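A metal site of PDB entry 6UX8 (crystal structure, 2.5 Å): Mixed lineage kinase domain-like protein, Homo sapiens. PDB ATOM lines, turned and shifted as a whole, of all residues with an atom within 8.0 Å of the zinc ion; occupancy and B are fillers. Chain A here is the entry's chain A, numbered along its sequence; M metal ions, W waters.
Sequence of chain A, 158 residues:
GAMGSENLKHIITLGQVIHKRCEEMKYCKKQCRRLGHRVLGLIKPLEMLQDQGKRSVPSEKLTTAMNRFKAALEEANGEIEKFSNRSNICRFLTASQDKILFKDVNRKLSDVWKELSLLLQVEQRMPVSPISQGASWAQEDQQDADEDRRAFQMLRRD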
ATOM      1  N   HIS A  19      -4.927  -7.048  16.332  1.00  0.00           N
ATOM      2  CA  HIS A  19      -5.338  -6.799  17.708  1.00  0.00           C
ATOM      3  C   HIS A  19      -4.445  -7.525  18.711  1.00  0.00           C
ATOM      4  O   HIS A  19      -4.142  -6.994  19.775  1.00  0.00           O
ATOM      5  CB  HIS A  19      -6.806  -7.208  17.899  1.00  0.00           C
ATOM      6  CG  HIS A  19      -7.256  -7.170  19.326  1.00  0.00           C
ATOM      7  ND1 HIS A  19      -7.598  -8.314  20.025  1.00  0.00           N
ATOM      8  CD2 HIS A  19      -7.399  -6.147  20.190  1.00  0.00           C
ATOM      9  CE1 HIS A  19      -7.953  -7.984  21.254  1.00  0.00           C
ATOM     10  NE2 HIS A  19      -7.836  -6.675  21.380  1.00  0.00           N
ATOM     11  N   LYS A  20      -4.021  -8.743  18.377  1.00  0.00           N
ATOM     12  CA  LYS A  20      -3.169  -9.502  19.279  1.00  0.00           C
ATOM     13  C   LYS A  20      -1.791  -8.857  19.405  1.00  0.00           C
ATOM     14  O   LYS A  20      -1.190  -8.866  20.483  1.00  0.00           O
ATOM     15  CB  LYS A  20      -3.038 -10.941  18.804  1.00  0.00           C
ATOM     16  N   CYS A  22      -1.167  -5.607  19.078  1.00  0.00           N
ATOM     17  CA  CYS A  22      -1.305  -4.358  19.836  1.00  0.00           C
ATOM     18  C   CYS A  22      -1.285  -4.620  21.330  1.00  0.00           C
ATOM     19  O   CYS A  22      -0.744  -3.806  22.101  1.00  0.00           O
ATOM     20  CB  CYS A  22      -2.589  -3.641  19.430  1.00  0.00           C
ATOM     21  SG  CYS A  22      -2.569  -2.947  17.759  1.00  0.00           S
ATOM     22  N   GLU A  23      -1.858  -5.742  21.779  1.00  0.00           N
ATOM     23  CA  GLU A  23      -1.836  -6.081  23.193  1.00  0.00           C
ATOM     24  C   GLU A  23      -0.432  -6.410  23.672  1.00  0.00           C
ATOM     25  O   GLU A  23      -0.144  -6.272  24.864  1.00  0.00           O
ATOM     26  CB  GLU A  23      -2.767  -7.256  23.465  1.00  0.00           C
ATOM     27  CG  GLU A  23      -4.205  -7.065  23.004  1.00  0.00           C
ATOM     28  CD  GLU A  23      -4.991  -6.131  23.903  1.00  0.00           C
ATOM     29  OE1 GLU A  23      -6.071  -5.653  23.463  1.00  0.00           O
ATOM     30  OE2 GLU A  23      -4.555  -5.882  25.045  1.00  0.00           O
ATOM     31  N   CYS A  32      -1.910   1.908  21.154  1.00  0.00           N
ATOM     32  CA  CYS A  32      -1.879   0.594  20.519  1.00  0.00           C
ATOM     33  C   CYS A  32      -3.181  -0.168  20.778  1.00  0.00           C
ATOM     34  O   CYS A  32      -3.791  -0.699  19.842  1.00  0.00           O
ATOM     35  CB  CYS A  32      -0.680  -0.212  21.013  1.00  0.00           C
ATOM     36  SG  CYS A  32       0.912   0.571  20.691  1.00  0.00           S
ATOM     37  N   ARG A  33      -3.612  -0.225  22.041  1.00  0.00           N
ATOM     38  CA  ARG A  33      -4.859  -0.912  22.344  1.00  0.00           C
ATOM     39  C   ARG A  33      -6.063  -0.199  21.740  1.00  0.00           C
ATOM     40  O   ARG A  33      -7.100  -0.832  21.485  1.00  0.00           O
ATOM     41  CB  ARG A  33      -5.023  -1.054  23.857  1.00  0.00           C
ATOM     42  CG  ARG A  33      -3.870  -1.760  24.548  1.00  0.00           C
ATOM     43  CD  ARG A  33      -4.110  -1.941  26.033  1.00  0.00           C
ATOM     44  NE  ARG A  33      -4.988  -3.079  26.314  1.00  0.00           N
ATOM     45  CZ  ARG A  33      -6.293  -2.994  26.527  1.00  0.00           C
ATOM     46  NH1 ARG A  33      -6.905  -1.816  26.489  1.00  0.00           N
ATOM     47  NH2 ARG A  33      -7.009  -4.090  26.769  1.00  0.00           N
ATOM     48  N   ARG A  34      -5.937   1.109  21.491  1.00  0.00           N
ATOM     49  CA  ARG A  34      -6.994   1.832  20.794  1.00  0.00           C
ATOM     50  C   ARG A  34      -7.077   1.402  19.329  1.00  0.00           C
ATOM     51  O   ARG A  34      -8.177   1.248  18.791  1.00  0.00           O
ATOM     52  CB  ARG A  34      -6.755   3.339  20.892  1.00  0.00           C
ATOM     53  CG  ARG A  34      -7.799   4.194  20.188  1.00  0.00           C
ATOM     54  CD  ARG A  34      -9.064   4.318  21.018  1.00  0.00           C
ATOM     55  NE  ARG A  34      -8.815   5.045  22.259  1.00  0.00           N
ATOM     56  CZ  ARG A  34      -9.757   5.347  23.142  1.00  0.00           C
ATOM     57  NH1 ARG A  34     -11.022   4.981  22.927  1.00  0.00           N
ATOM     58  NH2 ARG A  34      -9.447   6.008  24.249  1.00  0.00           N
ATOM     59  N   GLY A  36      -5.962  -1.565  17.943  1.00  0.00           N
ATOM     60  CA  GLY A  36      -6.398  -2.944  17.826  1.00  0.00           C
ATOM     61  C   GLY A  36      -7.874  -3.140  18.092  1.00  0.00           C
ATOM     62  O   GLY A  36      -8.513  -4.004  17.485  1.00  0.00           O
ATOM     63  N   HIS A  37      -8.444  -2.337  18.999  1.00  0.00           N
ATOM     64  CA  HIS A  37      -9.864  -2.446  19.290  1.00  0.00           C
ATOM     65  C   HIS A  37     -10.720  -1.786  18.216  1.00  0.00           C
ATOM     66  O   HIS A  37     -11.864  -2.205  17.994  1.00  0.00           O
ATOM     67  CB  HIS A  37     -10.171  -1.840  20.667  1.00  0.00           C
ATOM     68  CG  HIS A  37      -9.615  -2.642  21.802  1.00  0.00           C
ATOM     69  ND1 HIS A  37      -9.394  -2.106  23.055  1.00  0.00           N
ATOM     70  CD2 HIS A  37      -9.250  -3.944  21.878  1.00  0.00           C
ATOM     71  CE1 HIS A  37      -8.911  -3.035  23.849  1.00  0.00           C
ATOM     72  NE2 HIS A  37      -8.807  -4.167  23.158  1.00  0.00           N
ATOM     73  N   LEU A  40     -10.953  -4.435  15.607  1.00  0.00           N
ATOM     74  CA  LEU A  40     -11.947  -5.427  15.995  1.00  0.00           C
ATOM     75  C   LEU A  40     -13.358  -4.952  15.665  1.00  0.00           C
ATOM     76  O   LEU A  40     -14.215  -5.744  15.256  1.00  0.00           O
ATOM     77  CB  LEU A  40     -11.830  -5.756  17.483  1.00  0.00           C
ATOM     78  CG  LEU A  40     -10.613  -6.553  17.936  1.00  0.00           C
ATOM     79  CD1 LEU A  40     -10.721  -6.862  19.416  1.00  0.00           C
ATOM     80  CD2 LEU A  40     -10.478  -7.828  17.126  1.00  0.00           C
HETATM   81 ZN    ZN M   1      -8.020  -6.036  23.305  1.00  0.00          ZN
HETATM   82  O   HOH W   1      -8.342  -7.483  24.777  1.00  0.00           O
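Three residues have an atom within 4 Å of the zinc ion: His 19, Glu 23 and His 37.
Along chain A the residues within 4 Å of the zinc ion span positions 19 to 37.
The nearest printed residue that does not touch the zinc ion is Arg 33 (4.1 Å).
The side-chain carboxylate (OE2) of Glu 23 is in salt-bridge range of the guanidinium group (NE) of Arg 33, at 3.1 Å.
A ring nitrogen (ND1) of His 37 sits at hydrogen-bond distance from the backbone carbonyl oxygen of Arg 33, at 3.1 Å.
The zinc ion is bound by the side-chain carboxylate (OE1) of Glu 23 (2.0 Å), a ring nitrogen (NE2) of His 37 (2.0 Å), a ring nitrogen (NE2) of His 19 (2.0 Å) and water W1 (2.1 Å).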
